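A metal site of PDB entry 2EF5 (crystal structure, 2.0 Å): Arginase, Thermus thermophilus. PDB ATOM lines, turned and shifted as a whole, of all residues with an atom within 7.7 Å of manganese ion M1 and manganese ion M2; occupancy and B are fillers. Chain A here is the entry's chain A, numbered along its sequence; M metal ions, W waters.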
ATOM      1  N   ASP A  95       7.870  -0.417 -12.304  1.00  0.00           N
ATOM      2  CA  ASP A  95       6.630  -1.166 -12.113  1.00  0.00           C
ATOM      3  C   ASP A  95       6.346  -2.198 -13.183  1.00  0.00           C
ATOM      4  O   ASP A  95       6.550  -1.951 -14.374  1.00  0.00           O
ATOM      5  CB  ASP A  95       5.426  -0.232 -12.074  1.00  0.00           C
ATOM      6  CG  ASP A  95       5.523   0.812 -10.990  1.00  0.00           C
ATOM      7  OD1 ASP A  95       6.010   0.474  -9.890  1.00  0.00           O
ATOM      8  OD2 ASP A  95       5.087   1.955 -11.228  1.00  0.00           O
ATOM      9  N   HIS A  96       5.811  -3.343 -12.763  1.00  0.00           N
ATOM     10  CA  HIS A  96       5.454  -4.397 -13.700  1.00  0.00           C
ATOM     11  C   HIS A  96       4.261  -3.942 -14.549  1.00  0.00           C
ATOM     12  O   HIS A  96       3.909  -4.586 -15.528  1.00  0.00           O
ATOM     13  CB  HIS A  96       5.076  -5.664 -12.935  1.00  0.00           C
ATOM     14  CG  HIS A  96       5.360  -6.921 -13.702  1.00  0.00           C
ATOM     15  ND1 HIS A  96       5.506  -8.149 -13.084  1.00  0.00           N
ATOM     16  CD2 HIS A  96       5.579  -7.117 -15.016  1.00  0.00           C
ATOM     17  CE1 HIS A  96       5.824  -9.045 -14.002  1.00  0.00           C
ATOM     18  NE2 HIS A  96       5.878  -8.459 -15.173  1.00  0.00           N
ATOM     19  N   SER A  97       3.661  -2.821 -14.161  1.00  0.00           N
ATOM     20  CA  SER A  97       2.523  -2.252 -14.882  1.00  0.00           C
ATOM     21  C   SER A  97       2.903  -2.006 -16.340  1.00  0.00           C
ATOM     22  O   SER A  97       2.055  -2.066 -17.220  1.00  0.00           O
ATOM     23  CB  SER A  97       2.091  -0.921 -14.262  1.00  0.00           C
ATOM     24  OG  SER A  97       1.655  -1.082 -12.933  1.00  0.00           O
ATOM     25  N   SER A  99       4.203  -3.817 -18.345  1.00  0.00           N
ATOM     26  CA  SER A  99       3.940  -4.976 -19.186  1.00  0.00           C
ATOM     27  C   SER A  99       2.640  -4.878 -19.978  1.00  0.00           C
ATOM     28  O   SER A  99       2.489  -5.558 -20.986  1.00  0.00           O
ATOM     29  CB  SER A  99       3.947  -6.262 -18.352  1.00  0.00           C
ATOM     30  OG  SER A  99       5.279  -6.586 -17.947  1.00  0.00           O
ATOM     31  N   TRP A 116       4.947 -15.625 -17.415  1.00  0.00           N
ATOM     32  CA  TRP A 116       5.071 -14.643 -16.334  1.00  0.00           C
ATOM     33  C   TRP A 116       5.837 -15.270 -15.183  1.00  0.00           C
ATOM     34  O   TRP A 116       5.312 -16.131 -14.461  1.00  0.00           O
ATOM     35  CB  TRP A 116       3.657 -14.216 -15.916  1.00  0.00           C
ATOM     36  CG  TRP A 116       3.526 -12.881 -15.230  1.00  0.00           C
ATOM     37  CD1 TRP A 116       3.575 -12.640 -13.879  1.00  0.00           C
ATOM     38  CD2 TRP A 116       3.250 -11.613 -15.861  1.00  0.00           C
ATOM     39  NE1 TRP A 116       3.334 -11.300 -13.631  1.00  0.00           N
ATOM     40  CE2 TRP A 116       3.128 -10.662 -14.801  1.00  0.00           C
ATOM     41  CE3 TRP A 116       3.077 -11.216 -17.185  1.00  0.00           C
ATOM     42  CZ2 TRP A 116       2.850  -9.304 -15.078  1.00  0.00           C
ATOM     43  CZ3 TRP A 116       2.811  -9.854 -17.444  1.00  0.00           C
ATOM     44  CH2 TRP A 116       2.686  -8.920 -16.384  1.00  0.00           C
ATOM     45  N   VAL A 117       7.089 -14.869 -15.035  1.00  0.00           N
ATOM     46  CA  VAL A 117       7.982 -15.424 -14.003  1.00  0.00           C
ATOM     47  C   VAL A 117       7.996 -14.382 -12.902  1.00  0.00           C
ATOM     48  O   VAL A 117       8.682 -13.364 -12.983  1.00  0.00           O
ATOM     49  CB  VAL A 117       9.383 -15.674 -14.610  1.00  0.00           C
ATOM     50  CG1 VAL A 117      10.197 -16.567 -13.706  1.00  0.00           C
ATOM     51  CG2 VAL A 117       9.223 -16.289 -15.996  1.00  0.00           C
ATOM     52  N   ASP A 118       7.247 -14.697 -11.849  1.00  0.00           N
ATOM     53  CA  ASP A 118       7.024 -13.734 -10.778  1.00  0.00           C
ATOM     54  C   ASP A 118       6.648 -14.432  -9.478  1.00  0.00           C
ATOM     55  O   ASP A 118       6.090 -15.525  -9.501  1.00  0.00           O
ATOM     56  CB  ASP A 118       5.835 -12.906 -11.245  1.00  0.00           C
ATOM     57  CG  ASP A 118       5.762 -11.563 -10.604  1.00  0.00           C
ATOM     58  OD1 ASP A 118       5.881 -11.453  -9.363  1.00  0.00           O
ATOM     59  OD2 ASP A 118       5.535 -10.614 -11.381  1.00  0.00           O
ATOM     60  N   ALA A 119       6.923 -13.775  -8.354  1.00  0.00           N
ATOM     61  CA  ALA A 119       6.546 -14.333  -7.060  1.00  0.00           C
ATOM     62  C   ALA A 119       5.052 -14.063  -6.888  1.00  0.00           C
ATOM     63  O   ALA A 119       4.392 -14.691  -6.057  1.00  0.00           O
ATOM     64  CB  ALA A 119       7.326 -13.672  -5.935  1.00  0.00           C
ATOM     65  N   HIS A 120       4.529 -13.127  -7.672  1.00  0.00           N
ATOM     66  CA  HIS A 120       3.112 -12.779  -7.613  1.00  0.00           C
ATOM     67  C   HIS A 120       2.453 -13.057  -8.966  1.00  0.00           C
ATOM     68  O   HIS A 120       3.148 -13.240  -9.968  1.00  0.00           O
ATOM     69  CB  HIS A 120       2.925 -11.300  -7.256  1.00  0.00           C
ATOM     70  CG  HIS A 120       3.645 -10.900  -6.014  1.00  0.00           C
ATOM     71  ND1 HIS A 120       4.949 -10.444  -6.017  1.00  0.00           N
ATOM     72  CD2 HIS A 120       3.260 -10.933  -4.714  1.00  0.00           C
ATOM     73  CE1 HIS A 120       5.335 -10.212  -4.769  1.00  0.00           C
ATOM     74  NE2 HIS A 120       4.335 -10.509  -3.959  1.00  0.00           N
ATOM     75  N   ALA A 121       1.129 -13.060  -8.989  1.00  0.00           N
ATOM     76  CA  ALA A 121       0.381 -13.329 -10.214  1.00  0.00           C
ATOM     77  C   ALA A 121      -0.048 -12.065 -10.938  1.00  0.00           C
ATOM     78  O   ALA A 121      -0.367 -12.117 -12.132  1.00  0.00           O
ATOM     79  CB  ALA A 121      -0.849 -14.180  -9.893  1.00  0.00           C
ATOM     80  N   ASP A 122      -0.051 -10.939 -10.242  1.00  0.00           N
ATOM     81  CA  ASP A 122      -0.453  -9.657 -10.829  1.00  0.00           C
ATOM     82  C   ASP A 122      -1.753  -9.835 -11.591  1.00  0.00           C
ATOM     83  O   ASP A 122      -1.938  -9.270 -12.671  1.00  0.00           O
ATOM     84  CB  ASP A 122       0.620  -9.134 -11.781  1.00  0.00           C
ATOM     85  CG  ASP A 122       1.932  -8.842 -11.095  1.00  0.00           C
ATOM     86  OD1 ASP A 122       1.917  -8.330  -9.949  1.00  0.00           O
ATOM     87  OD2 ASP A 122       2.994  -9.131 -11.688  1.00  0.00           O
ATOM     88  N   HIS A 135       0.158  -1.911 -10.528  1.00  0.00           N
ATOM     89  CA  HIS A 135       1.209  -2.868 -10.831  1.00  0.00           C
ATOM     90  C   HIS A 135       0.896  -4.259 -10.288  1.00  0.00           C
ATOM     91  O   HIS A 135       1.695  -5.189 -10.412  1.00  0.00           O
ATOM     92  CB  HIS A 135       2.571  -2.362 -10.340  1.00  0.00           C
ATOM     93  CG  HIS A 135       2.596  -1.930  -8.898  1.00  0.00           C
ATOM     94  ND1 HIS A 135       2.434  -2.810  -7.854  1.00  0.00           N
ATOM     95  CD2 HIS A 135       2.828  -0.716  -8.345  1.00  0.00           C
ATOM     96  CE1 HIS A 135       2.570  -2.154  -6.713  1.00  0.00           C
ATOM     97  NE2 HIS A 135       2.811  -0.887  -6.982  1.00  0.00           N
ATOM     98  N   GLY A 136      -0.289  -4.403  -9.701  1.00  0.00           N
ATOM     99  CA  GLY A 136      -0.713  -5.685  -9.179  1.00  0.00           C
ATOM    100  C   GLY A 136      -1.853  -6.217 -10.034  1.00  0.00           C
ATOM    101  O   GLY A 136      -2.527  -7.172  -9.668  1.00  0.00           O
ATOM    102  N   PRO A 138      -1.515  -5.866 -13.969  1.00  0.00           N
ATOM    103  CA  PRO A 138      -1.175  -5.984 -15.397  1.00  0.00           C
ATOM    104  C   PRO A 138      -1.504  -7.273 -16.150  1.00  0.00           C
ATOM    105  O   PRO A 138      -1.952  -7.213 -17.288  1.00  0.00           O
ATOM    106  CB  PRO A 138       0.321  -5.668 -15.423  1.00  0.00           C
ATOM    107  CG  PRO A 138       0.796  -6.203 -14.117  1.00  0.00           C
ATOM    108  CD  PRO A 138      -0.283  -5.717 -13.168  1.00  0.00           C
ATOM    109  N   SER A 215       8.094 -12.361 -19.239  1.00  0.00           N
ATOM    110  CA  SER A 215       8.076 -11.209 -18.358  1.00  0.00           C
ATOM    111  C   SER A 215       8.715 -11.648 -17.053  1.00  0.00           C
ATOM    112  O   SER A 215       8.125 -12.427 -16.296  1.00  0.00           O
ATOM    113  CB  SER A 215       6.633 -10.727 -18.136  1.00  0.00           C
ATOM    114  OG  SER A 215       6.627  -9.428 -17.603  1.00  0.00           O
ATOM    115  N   LEU A 216       9.914 -11.159 -16.798  1.00  0.00           N
ATOM    116  CA  LEU A 216      10.656 -11.541 -15.604  1.00  0.00           C
ATOM    117  C   LEU A 216      10.676 -10.501 -14.490  1.00  0.00           C
ATOM    118  O   LEU A 216      11.268  -9.426 -14.628  1.00  0.00           O
ATOM    119  CB  LEU A 216      12.089 -11.923 -16.009  1.00  0.00           C
ATOM    120  CG  LEU A 216      13.105 -12.328 -14.932  1.00  0.00           C
ATOM    121  CD1 LEU A 216      12.618 -13.563 -14.181  1.00  0.00           C
ATOM    122  CD2 LEU A 216      14.452 -12.625 -15.615  1.00  0.00           C
ATOM    123  N   ASP A 217      10.006 -10.817 -13.392  1.00  0.00           N
ATOM    124  CA  ASP A 217       9.958  -9.952 -12.225  1.00  0.00           C
ATOM    125  C   ASP A 217      11.105 -10.421 -11.321  1.00  0.00           C
ATOM    126  O   ASP A 217      11.177 -11.593 -10.989  1.00  0.00           O
ATOM    127  CB  ASP A 217       8.627 -10.098 -11.483  1.00  0.00           C
ATOM    128  CG  ASP A 217       8.470  -9.087 -10.372  1.00  0.00           C
ATOM    129  OD1 ASP A 217       9.427  -8.882  -9.610  1.00  0.00           O
ATOM    130  OD2 ASP A 217       7.382  -8.487 -10.254  1.00  0.00           O
ATOM    131  N   ALA A 218      11.979  -9.500 -10.952  1.00  0.00           N
ATOM    132  CA  ALA A 218      13.126  -9.826 -10.117  1.00  0.00           C
ATOM    133  C   ALA A 218      12.750 -10.535  -8.825  1.00  0.00           C
ATOM    134  O   ALA A 218      13.532 -11.326  -8.302  1.00  0.00           O
ATOM    135  CB  ALA A 218      13.923  -8.566  -9.788  1.00  0.00           C
ATOM    136  N   ASP A 219      11.545 -10.264  -8.308  1.00  0.00           N
ATOM    137  CA  ASP A 219      11.152 -10.875  -7.061  1.00  0.00           C
ATOM    138  C   ASP A 219      10.860 -12.368  -7.109  1.00  0.00           C
ATOM    139  O   ASP A 219      10.541 -12.952  -6.094  1.00  0.00           O
ATOM    140  CB  ASP A 219       9.960 -10.140  -6.437  1.00  0.00           C
ATOM    141  CG  ASP A 219       8.651 -10.395  -7.158  1.00  0.00           C
ATOM    142  OD1 ASP A 219       8.570 -11.297  -8.011  1.00  0.00           O
ATOM    143  OD2 ASP A 219       7.672  -9.692  -6.842  1.00  0.00           O
ATOM    144  N   VAL A 220      10.966 -12.984  -8.287  1.00  0.00           N
ATOM    145  CA  VAL A 220      10.716 -14.427  -8.377  1.00  0.00           C
ATOM    146  C   VAL A 220      11.910 -15.149  -7.749  1.00  0.00           C
ATOM    147  O   VAL A 220      11.789 -16.264  -7.265  1.00  0.00           O
ATOM    148  CB  VAL A 220      10.553 -14.891  -9.853  1.00  0.00           C
ATOM    149  CG1 VAL A 220      11.895 -14.853 -10.573  1.00  0.00           C
ATOM    150  CG2 VAL A 220       9.963 -16.288  -9.888  1.00  0.00           C
ATOM    151  N   VAL A 229      14.213  -5.712  -4.399  1.00  0.00           N
ATOM    152  CA  VAL A 229      12.849  -5.791  -4.918  1.00  0.00           C
ATOM    153  C   VAL A 229      11.859  -5.191  -3.923  1.00  0.00           C
ATOM    154  O   VAL A 229      12.056  -5.276  -2.711  1.00  0.00           O
ATOM    155  CB  VAL A 229      12.430  -7.259  -5.212  1.00  0.00           C
ATOM    156  CG1 VAL A 229      13.426  -7.897  -6.184  1.00  0.00           C
ATOM    157  CG2 VAL A 229      12.373  -8.062  -3.926  1.00  0.00           C
ATOM    158  N   THR A 231       8.609  -6.045  -3.192  1.00  0.00           N
ATOM    159  CA  THR A 231       7.852  -6.991  -2.388  1.00  0.00           C
ATOM    160  C   THR A 231       8.519  -8.358  -2.318  1.00  0.00           C
ATOM    161  O   THR A 231       8.091  -9.315  -2.965  1.00  0.00           O
ATOM    162  CB  THR A 231       6.418  -7.141  -2.942  1.00  0.00           C
ATOM    163  OG1 THR A 231       5.879  -5.842  -3.215  1.00  0.00           O
ATOM    164  CG2 THR A 231       5.530  -7.837  -1.937  1.00  0.00           C
ATOM    165  N   VAL A 233       9.571 -12.026  -1.154  1.00  0.00           N
ATOM    166  CA  VAL A 233       8.837 -13.138  -0.576  1.00  0.00           C
ATOM    167  C   VAL A 233       9.815 -14.308  -0.468  1.00  0.00           C
ATOM    168  O   VAL A 233      10.367 -14.757  -1.482  1.00  0.00           O
ATOM    169  CB  VAL A 233       7.638 -13.549  -1.456  1.00  0.00           C
ATOM    170  CG1 VAL A 233       6.800 -14.586  -0.729  1.00  0.00           C
ATOM    171  CG2 VAL A 233       6.805 -12.319  -1.804  1.00  0.00           C
ATOM    172  N   VAL A 261      11.746  -6.514 -15.016  1.00  0.00           N
ATOM    173  CA  VAL A 261      11.113  -5.539 -14.142  1.00  0.00           C
ATOM    174  C   VAL A 261      11.329  -5.661 -12.645  1.00  0.00           C
ATOM    175  O   VAL A 261      11.905  -6.621 -12.151  1.00  0.00           O
ATOM    176  CB  VAL A 261       9.573  -5.554 -14.372  1.00  0.00           C
ATOM    177  CG1 VAL A 261       9.247  -5.315 -15.845  1.00  0.00           C
ATOM    178  CG2 VAL A 261       9.006  -6.901 -13.923  1.00  0.00           C
ATOM    179  N   GLU A 262      10.829  -4.640 -11.948  1.00  0.00           N
ATOM    180  CA  GLU A 262      10.858  -4.537 -10.490  1.00  0.00           C
ATOM    181  C   GLU A 262      12.220  -4.491  -9.789  1.00  0.00           C
ATOM    182  O   GLU A 262      12.316  -4.749  -8.596  1.00  0.00           O
ATOM    183  CB  GLU A 262      10.005  -5.668  -9.905  1.00  0.00           C
ATOM    184  CG  GLU A 262       8.513  -5.587 -10.281  1.00  0.00           C
ATOM    185  CD  GLU A 262       7.749  -4.514  -9.505  1.00  0.00           C
ATOM    186  OE1 GLU A 262       8.002  -4.355  -8.297  1.00  0.00           O
ATOM    187  OE2 GLU A 262       6.898  -3.821 -10.096  1.00  0.00           O
HETATM  188 MN    MN M   1       6.088  -9.480  -8.366  1.00  0.00          MN
HETATM  189 MN    MN M   2       5.046  -8.615 -10.978  1.00  0.00          MN
HETATM  190  O   HOH W   1       4.915  -6.511  -7.895  1.00  0.00           O
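N of His 120 lies close to OD1 of Asp 118.
The side-chain carboxylate (OE2) of Glu 262 is in hydrogen-bond range of the backbone NH (N) of His 96 (2.9 Å).
NE2 of His 96 is in hydrogen-bond range of OG of Ser 215 (2.7 Å).
OG of Ser 99 sits close to NE2 of His 96.
ND1 of His 120 lies close to OD2 of Asp 219.
The side-chain carboxylate (OD1) of Asp 219 sits at hydrogen-bond distance from the backbone NH (N) of Ala 119.
The indole nitrogen (NE1) of Trp 116 sits close to the side-chain carboxylate (OD2) of Asp 122.
N of Asp 217 lies within hydrogen-bond range of O of Val 117, at 2.9 Å.
Manganese ion M2 is bound by the side-chain carboxylate of Asp 118 (2.1 Å), a ring nitrogen (ND1) of His 96 (2.2 Å), the side-chain carboxylate of Asp 122 (2.2 Å) and the side-chain carboxylate of Asp 217 (2.4 Å).
The nearest printed residue that does not touch manganese ion M2 is Trp 116 (4.1 Å).
Manganese ion M1 is bound by the side-chain carboxylate of Asp 219 (2.2 Å), the side-chain carboxylate of Asp 118 (2.2 Å) and the side-chain carboxylate of Asp 217 (2.5 Å).
Slightly farther from manganese ion M1 lies ND1 of His 120 (2.8 Å).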
